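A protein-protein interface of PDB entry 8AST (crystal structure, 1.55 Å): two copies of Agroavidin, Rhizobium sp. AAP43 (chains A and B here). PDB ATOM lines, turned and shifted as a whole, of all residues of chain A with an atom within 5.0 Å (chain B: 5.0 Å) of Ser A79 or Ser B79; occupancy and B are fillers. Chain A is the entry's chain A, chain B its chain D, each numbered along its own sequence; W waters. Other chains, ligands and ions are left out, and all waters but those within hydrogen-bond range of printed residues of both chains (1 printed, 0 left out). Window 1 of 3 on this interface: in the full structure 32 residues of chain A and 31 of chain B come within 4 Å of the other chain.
Water W1 lies within hydrogen-bond range of OG of Ser B64 (2.7 Å) and OG of Ser A64 (3.0 Å).
Hydrophobic or aromatic side chains of chain B that line the printed part of chain A: Ala B62, Ala B77 and Ala B81.
Hydrophobic or aromatic side chains of chain A within 4 Å of the printed part of chain B: Ala A62, Ala A77 and Ala A81.
Among the printed residues, 21 pairs touch across the chains.
Among the printed residues, no Asp or Glu carboxylate lies within 4 Å of a Lys or Arg side-chain nitrogen of the other chain.
Among the printed residues, merely in contact across the chains: Ala A81 with Ser B99, Ser A64 with Ala B62, Ser A99 with Ala B81, Trp A98 with Ser B99, Ala A62 with Ser B64, Ser A99 with Trp B98, Ala A62 with Thr B78, Ala A77 with Ala B81, Ala A81 with Ser B79, Ser A79 with Ala B81, Ala A81 with Ala B77, Ala A62 with Ala B77, Ala A77 with Ala B62 and Ala A62 with Ser B79.
Of the printed residues of chain B, Ser A79 touches Ser B79 (2.9 Å), Trp B80 (3.4 Å) and Ala B81 (3.6 Å).
Of the printed residues of chain B, Ala A77 touches Ala B62 and Ala B81.
Printed residues of chain B within 4 Å of Phe A63: Ser B64 (3.5 Å).
Of the printed residues of chain B, Ala A62 touches Ser B64, Ala B77, Thr B78 and Ser B79.
Printed residues of chain A within 4 Å of Thr B78: Ala A62 (3.6 Å).
Phe B63 touches none of the printed residues of chain A.
The nearest printed residue of chain B that does not touch Ser A79 is Ser B99 (4.1 Å).
O of Phe A63 is in hydrogen-bond range of N of Trp A80 (2.8 Å).
The backbone carbonyl oxygen (O) of Ser A79 is in hydrogen-bond range of the backbone NH (N) of Ser A99 (2.8 Å).
The backbone carbonyl oxygen (O) of Ala A81 is in hydrogen-bond range of the backbone NH (N) of Gln A97, 2.9 Å away.
O of Phe B63 is in hydrogen-bond range of N of Trp B80 (2.8 Å).
The backbone carbonyl oxygen (O) of Ser B79 sits at hydrogen-bond distance from the backbone NH (N) of Ser B99 (2.8 Å).
O of Ala B81 is in hydrogen-bond range of N of Gln B97.
Ala A62 touches Thr B78, but with the chains exchanged Thr A78 does not touch Ala B62 (4.2 Å).
Ser A79 touches its own counterpart, Ser B79.
Ser A79 touches Trp B80, and with the chains exchanged Trp A80 touches Ser B79.
Ser A79 touches Ala B81, and with the chains exchanged Ala A81 touches Ser B79.
11 positions are printed for both chains.
The backbone NH (N) of Phe A63 is in hydrogen-bond range of the side-chain hydroxyl (OG) of Ser B64, 3.5 Å away.
OG of Ser A79 is in hydrogen-bond range of OG of Ser B79, 2.9 Å away.
OG of Ser A79 lies close to N of Trp B80, 3.5 Å away.
OG of Ser B79 is in hydrogen-bond range of O of Trp A80, at 3.0 Å.
The backbone carbonyl oxygen (O) of Gln A97 sits at hydrogen-bond distance from the side-chain hydroxyl (OG) of Ser B99 (3.2 Å).
The side-chain hydroxyl (OG) of Ser A99 sits at hydrogen-bond distance from the backbone carbonyl oxygen (O) of Gln B97, 3.4 Å away.
OG of Ser B99 lies within hydrogen-bond range of OG of Ser A99 (2.6 Å).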
ATOM      1  N   ALA A  62      11.915  -5.398 -27.895  1.00  0.00           N
ATOM      2  CA  ALA A  62      12.181  -6.780 -28.323  1.00  0.00           C
ATOM      3  C   ALA A  62      13.544  -6.789 -28.970  1.00  0.00           C
ATOM      4  O   ALA A  62      13.854  -5.832 -29.706  1.00  0.00           O
ATOM      5  CB  ALA A  62      11.147  -7.353 -29.258  1.00  0.00           C
ATOM      6  N   PHE A  63      14.339  -7.803 -28.686  1.00  0.00           N
ATOM      7  CA  PHE A  63      15.707  -7.816 -29.240  1.00  0.00           C
ATOM      8  C   PHE A  63      16.164  -9.251 -29.292  1.00  0.00           C
ATOM      9  O   PHE A  63      15.598 -10.150 -28.655  1.00  0.00           O
ATOM     10  CB  PHE A  63      16.659  -6.938 -28.424  1.00  0.00           C
ATOM     11  CG  PHE A  63      16.788  -7.309 -26.986  1.00  0.00           C
ATOM     12  CD1 PHE A  63      15.972  -6.689 -26.052  1.00  0.00           C
ATOM     13  CD2 PHE A  63      17.761  -8.183 -26.541  1.00  0.00           C
ATOM     14  CE1 PHE A  63      16.056  -7.015 -24.707  1.00  0.00           C
ATOM     15  CE2 PHE A  63      17.885  -8.455 -25.189  1.00  0.00           C
ATOM     16  CZ  PHE A  63      17.007  -7.906 -24.287  1.00  0.00           C
ATOM     17  N   SER A  64      17.200  -9.493 -30.076  1.00  0.00           N
ATOM     18  CA  SER A  64      17.702 -10.871 -30.227  1.00  0.00           C
ATOM     19  C   SER A  64      19.204 -10.885 -30.421  1.00  0.00           C
ATOM     20  O   SER A  64      19.785  -9.877 -30.835  1.00  0.00           O
ATOM     21  CB  SER A  64      17.044 -11.578 -31.358  1.00  0.00           C
ATOM     22  OG  SER A  64      17.507 -11.089 -32.615  1.00  0.00           O
ATOM     23  N   ALA A  77      20.250 -19.176 -31.077  1.00  0.00           N
ATOM     24  CA  ALA A  77      19.706 -17.814 -31.157  1.00  0.00           C
ATOM     25  C   ALA A  77      18.769 -17.597 -29.983  1.00  0.00           C
ATOM     26  O   ALA A  77      17.993 -18.493 -29.608  1.00  0.00           O
ATOM     27  CB  ALA A  77      18.969 -17.604 -32.455  1.00  0.00           C
ATOM     28  N   THR A  78      18.854 -16.438 -29.378  1.00  0.00           N
ATOM     29  CA  THR A  78      17.956 -16.091 -28.274  1.00  0.00           C
ATOM     30  C   THR A  78      17.218 -14.830 -28.622  1.00  0.00           C
ATOM     31  O   THR A  78      17.809 -13.872 -29.115  1.00  0.00           O
ATOM     32  CB  THR A  78      18.723 -15.884 -26.963  1.00  0.00           C
ATOM     33  OG1 THR A  78      19.508 -17.059 -26.700  1.00  0.00           O
ATOM     34  CG2 THR A  78      17.792 -15.635 -25.806  1.00  0.00           C
ATOM     35  N   SER A  79      15.924 -14.806 -28.328  1.00  0.00           N
ATOM     36  CA  SER A  79      15.108 -13.591 -28.479  1.00  0.00           C
ATOM     37  C   SER A  79      14.504 -13.259 -27.116  1.00  0.00           C
ATOM     38  O   SER A  79      14.259 -14.179 -26.308  1.00  0.00           O
ATOM     39  CB  SER A  79      14.061 -13.780 -29.558  1.00  0.00           C
ATOM     40  OG  SER A  79      12.909 -14.400 -29.020  1.00  0.00           O
ATOM     41  N   TRP A  80      14.399 -11.965 -26.854  1.00  0.00           N
ATOM     42  CA  TRP A  80      13.743 -11.405 -25.668  1.00  0.00           C
ATOM     43  C   TRP A  80      12.653 -10.440 -26.075  1.00  0.00           C
ATOM     44  O   TRP A  80      12.788  -9.676 -27.039  1.00  0.00           O
ATOM     45  CB  TRP A  80      14.753 -10.652 -24.791  1.00  0.00           C
ATOM     46  CG  TRP A  80      15.846 -11.405 -24.117  1.00  0.00           C
ATOM     47  CD1 TRP A  80      15.940 -11.702 -22.787  1.00  0.00           C
ATOM     48  CD2 TRP A  80      17.096 -11.790 -24.705  1.00  0.00           C
ATOM     49  NE1 TRP A  80      17.133 -12.301 -22.514  1.00  0.00           N
ATOM     50  CE2 TRP A  80      17.878 -12.352 -23.672  1.00  0.00           C
ATOM     51  CE3 TRP A  80      17.648 -11.666 -25.980  1.00  0.00           C
ATOM     52  CZ2 TRP A  80      19.168 -12.814 -23.882  1.00  0.00           C
ATOM     53  CZ3 TRP A  80      18.924 -12.117 -26.186  1.00  0.00           C
ATOM     54  CH2 TRP A  80      19.663 -12.712 -25.145  1.00  0.00           C
ATOM     55  N   ALA A  81      11.562 -10.439 -25.293  1.00  0.00           N
ATOM     56  CA  ALA A  81      10.552  -9.372 -25.401  1.00  0.00           C
ATOM     57  C   ALA A  81      10.252  -8.932 -23.976  1.00  0.00           C
ATOM     58  O   ALA A  81      10.189  -9.804 -23.087  1.00  0.00           O
ATOM     59  CB  ALA A  81       9.287  -9.835 -26.105  1.00  0.00           C
ATOM     60  N   GLN A  97      10.663 -11.989 -21.219  1.00  0.00           N
ATOM     61  CA  GLN A  97      10.584 -13.425 -21.512  1.00  0.00           C
ATOM     62  C   GLN A  97      11.604 -13.692 -22.609  1.00  0.00           C
ATOM     63  O   GLN A  97      11.624 -12.884 -23.570  1.00  0.00           O
ATOM     64  CB  GLN A  97       9.180 -13.741 -22.029  1.00  0.00           C
ATOM     65  CG  GLN A  97       8.980 -15.180 -22.462  1.00  0.00           C
ATOM     66  CD  GLN A  97       8.791 -16.131 -21.307  1.00  0.00           C
ATOM     67  OE1 GLN A  97       9.002 -17.338 -21.436  1.00  0.00           O
ATOM     68  NE2 GLN A  97       8.446 -15.595 -20.160  1.00  0.00           N
ATOM     69  N   TRP A  98      12.363 -14.756 -22.532  1.00  0.00           N
ATOM     70  CA  TRP A  98      13.280 -15.150 -23.623  1.00  0.00           C
ATOM     71  C   TRP A  98      12.864 -16.493 -24.198  1.00  0.00           C
ATOM     72  O   TRP A  98      12.257 -17.326 -23.494  1.00  0.00           O
ATOM     73  CB  TRP A  98      14.752 -15.142 -23.188  1.00  0.00           C
ATOM     74  CG  TRP A  98      15.068 -15.983 -21.989  1.00  0.00           C
ATOM     75  CD1 TRP A  98      15.180 -15.555 -20.697  1.00  0.00           C
ATOM     76  CD2 TRP A  98      15.371 -17.390 -21.969  1.00  0.00           C
ATOM     77  NE1 TRP A  98      15.532 -16.592 -19.889  1.00  0.00           N
ATOM     78  CE2 TRP A  98      15.641 -17.736 -20.627  1.00  0.00           C
ATOM     79  CE3 TRP A  98      15.414 -18.393 -22.941  1.00  0.00           C
ATOM     80  CZ2 TRP A  98      15.947 -19.044 -20.244  1.00  0.00           C
ATOM     81  CZ3 TRP A  98      15.758 -19.677 -22.575  1.00  0.00           C
ATOM     82  CH2 TRP A  98      16.016 -20.000 -21.233  1.00  0.00           C
ATOM     83  N   SER A  99      13.189 -16.668 -25.465  1.00  0.00           N
ATOM     84  CA  SER A  99      13.094 -17.911 -26.242  1.00  0.00           C
ATOM     85  C   SER A  99      14.495 -18.248 -26.746  1.00  0.00           C
ATOM     86  O   SER A  99      15.189 -17.350 -27.294  1.00  0.00           O
ATOM     87  CB  SER A  99      12.152 -17.731 -27.407  1.00  0.00           C
ATOM     88  OG  SER A  99      11.023 -16.903 -27.091  1.00  0.00           O
ATOM     89  N   ALA B  62      16.718 -15.354 -35.396  1.00  0.00           N
ATOM     90  CA  ALA B  62      15.920 -14.626 -34.390  1.00  0.00           C
ATOM     91  C   ALA B  62      15.514 -13.295 -34.990  1.00  0.00           C
ATOM     92  O   ALA B  62      16.288 -12.741 -35.804  1.00  0.00           O
ATOM     93  CB  ALA B  62      16.689 -14.485 -33.123  1.00  0.00           C
ATOM     94  N   PHE B  63      14.300 -12.836 -34.675  1.00  0.00           N
ATOM     95  CA  PHE B  63      13.796 -11.579 -35.247  1.00  0.00           C
ATOM     96  C   PHE B  63      12.748 -11.005 -34.291  1.00  0.00           C
ATOM     97  O   PHE B  63      12.210 -11.746 -33.418  1.00  0.00           O
ATOM     98  CB  PHE B  63      13.311 -11.780 -36.682  1.00  0.00           C
ATOM     99  CG  PHE B  63      12.273 -12.845 -36.855  1.00  0.00           C
ATOM    100  CD1 PHE B  63      10.938 -12.517 -36.712  1.00  0.00           C
ATOM    101  CD2 PHE B  63      12.616 -14.158 -37.145  1.00  0.00           C
ATOM    102  CE1 PHE B  63       9.971 -13.486 -36.868  1.00  0.00           C
ATOM    103  CE2 PHE B  63      11.633 -15.130 -37.294  1.00  0.00           C
ATOM    104  CZ  PHE B  63      10.297 -14.786 -37.118  1.00  0.00           C
ATOM    105  N   SER B  64      12.549  -9.692 -34.426  1.00  0.00           N
ATOM    106  CA  SER B  64      11.719  -8.888 -33.509  1.00  0.00           C
ATOM    107  C   SER B  64      10.819  -7.958 -34.324  1.00  0.00           C
ATOM    108  O   SER B  64      11.261  -7.408 -35.356  1.00  0.00           O
ATOM    109  CB  SER B  64      12.631  -8.082 -32.558  1.00  0.00           C
ATOM    110  OG  SER B  64      13.452  -8.985 -31.815  1.00  0.00           O
ATOM    111  N   ALA B  77       5.351  -5.837 -28.194  1.00  0.00           N
ATOM    112  CA  ALA B  77       6.547  -6.252 -28.961  1.00  0.00           C
ATOM    113  C   ALA B  77       6.593  -7.751 -28.910  1.00  0.00           C
ATOM    114  O   ALA B  77       6.410  -8.334 -27.828  1.00  0.00           O
ATOM    115  CB  ALA B  77       7.805  -5.636 -28.395  1.00  0.00           C
ATOM    116  N   THR B  78       6.983  -8.332 -30.023  1.00  0.00           N
ATOM    117  CA  THR B  78       7.154  -9.789 -30.118  1.00  0.00           C
ATOM    118  C   THR B  78       8.562 -10.083 -30.636  1.00  0.00           C
ATOM    119  O   THR B  78       9.093  -9.335 -31.476  1.00  0.00           O
ATOM    120  CB  THR B  78       6.103 -10.428 -31.030  1.00  0.00           C
ATOM    121  OG1 THR B  78       4.795 -10.078 -30.530  1.00  0.00           O
ATOM    122  CG2 THR B  78       6.243 -11.926 -31.088  1.00  0.00           C
ATOM    123  N   SER B  79       9.178 -11.112 -30.076  1.00  0.00           N
ATOM    124  CA  SER B  79      10.426 -11.647 -30.642  1.00  0.00           C
ATOM    125  C   SER B  79      10.280 -13.160 -30.777  1.00  0.00           C
ATOM    126  O   SER B  79       9.607 -13.817 -29.955  1.00  0.00           O
ATOM    127  CB  SER B  79      11.625 -11.237 -29.870  1.00  0.00           C
ATOM    128  OG  SER B  79      11.598 -11.879 -28.642  1.00  0.00           O
ATOM    129  N   TRP B  80      10.947 -13.680 -31.791  1.00  0.00           N
ATOM    130  CA  TRP B  80      10.940 -15.100 -32.170  1.00  0.00           C
ATOM    131  C   TRP B  80      12.383 -15.596 -32.208  1.00  0.00           C
ATOM    132  O   TRP B  80      13.260 -14.878 -32.734  1.00  0.00           O
ATOM    133  CB  TRP B  80      10.352 -15.301 -33.571  1.00  0.00           C
ATOM    134  CG  TRP B  80       8.888 -15.019 -33.747  1.00  0.00           C
ATOM    135  CD1 TRP B  80       7.884 -15.942 -33.867  1.00  0.00           C
ATOM    136  CD2 TRP B  80       8.284 -13.745 -34.010  1.00  0.00           C
ATOM    137  NE1 TRP B  80       6.697 -15.321 -34.121  1.00  0.00           N
ATOM    138  CE2 TRP B  80       6.901 -13.973 -34.191  1.00  0.00           C
ATOM    139  CE3 TRP B  80       8.749 -12.423 -34.052  1.00  0.00           C
ATOM    140  CZ2 TRP B  80       6.017 -12.921 -34.467  1.00  0.00           C
ATOM    141  CZ3 TRP B  80       7.875 -11.390 -34.311  1.00  0.00           C
ATOM    142  CH2 TRP B  80       6.510 -11.645 -34.530  1.00  0.00           C
ATOM    143  N   ALA B  81      12.602 -16.812 -31.737  1.00  0.00           N
ATOM    144  CA  ALA B  81      13.843 -17.554 -31.978  1.00  0.00           C
ATOM    145  C   ALA B  81      13.462 -18.886 -32.623  1.00  0.00           C
ATOM    146  O   ALA B  81      12.499 -19.509 -32.161  1.00  0.00           O
ATOM    147  CB  ALA B  81      14.616 -17.785 -30.702  1.00  0.00           C
ATOM    148  N   GLN B  97       9.816 -20.304 -31.246  1.00  0.00           N
ATOM    149  CA  GLN B  97       9.169 -19.963 -29.971  1.00  0.00           C
ATOM    150  C   GLN B  97       9.173 -18.448 -29.946  1.00  0.00           C
ATOM    151  O   GLN B  97      10.212 -17.869 -30.249  1.00  0.00           O
ATOM    152  CB  GLN B  97       9.935 -20.569 -28.799  1.00  0.00           C
ATOM    153  CG  GLN B  97       9.352 -20.299 -27.418  1.00  0.00           C
ATOM    154  CD  GLN B  97       8.188 -21.209 -27.084  1.00  0.00           C
ATOM    155  OE1 GLN B  97       7.413 -20.933 -26.171  1.00  0.00           O
ATOM    156  NE2 GLN B  97       8.000 -22.247 -27.882  1.00  0.00           N
ATOM    157  N   TRP B  98       8.051 -17.854 -29.586  1.00  0.00           N
ATOM    158  CA  TRP B  98       7.923 -16.392 -29.496  1.00  0.00           C
ATOM    159  C   TRP B  98       7.672 -15.960 -28.057  1.00  0.00           C
ATOM    160  O   TRP B  98       7.150 -16.732 -27.267  1.00  0.00           O
ATOM    161  CB  TRP B  98       6.848 -15.855 -30.439  1.00  0.00           C
ATOM    162  CG  TRP B  98       5.497 -16.480 -30.293  1.00  0.00           C
ATOM    163  CD1 TRP B  98       4.978 -17.473 -31.070  1.00  0.00           C
ATOM    164  CD2 TRP B  98       4.458 -16.130 -29.349  1.00  0.00           C
ATOM    165  NE1 TRP B  98       3.704 -17.767 -30.665  1.00  0.00           N
ATOM    166  CE2 TRP B  98       3.362 -16.967 -29.605  1.00  0.00           C
ATOM    167  CE3 TRP B  98       4.352 -15.192 -28.314  1.00  0.00           C
ATOM    168  CZ2 TRP B  98       2.170 -16.876 -28.890  1.00  0.00           C
ATOM    169  CZ3 TRP B  98       3.199 -15.140 -27.561  1.00  0.00           C
ATOM    170  CH2 TRP B  98       2.121 -15.986 -27.842  1.00  0.00           C
ATOM    171  N   SER B  99       8.143 -14.758 -27.774  1.00  0.00           N
ATOM    172  CA  SER B  99       7.969 -14.034 -26.499  1.00  0.00           C
ATOM    173  C   SER B  99       7.162 -12.793 -26.864  1.00  0.00           C
ATOM    174  O   SER B  99       7.500 -12.105 -27.877  1.00  0.00           O
ATOM    175  CB  SER B  99       9.326 -13.643 -25.874  1.00  0.00           C
ATOM    176  OG  SER B  99      10.262 -14.724 -25.856  1.00  0.00           O
HETATM  177  O   HOH W   1      15.708  -8.827 -33.265  1.00  0.00           O
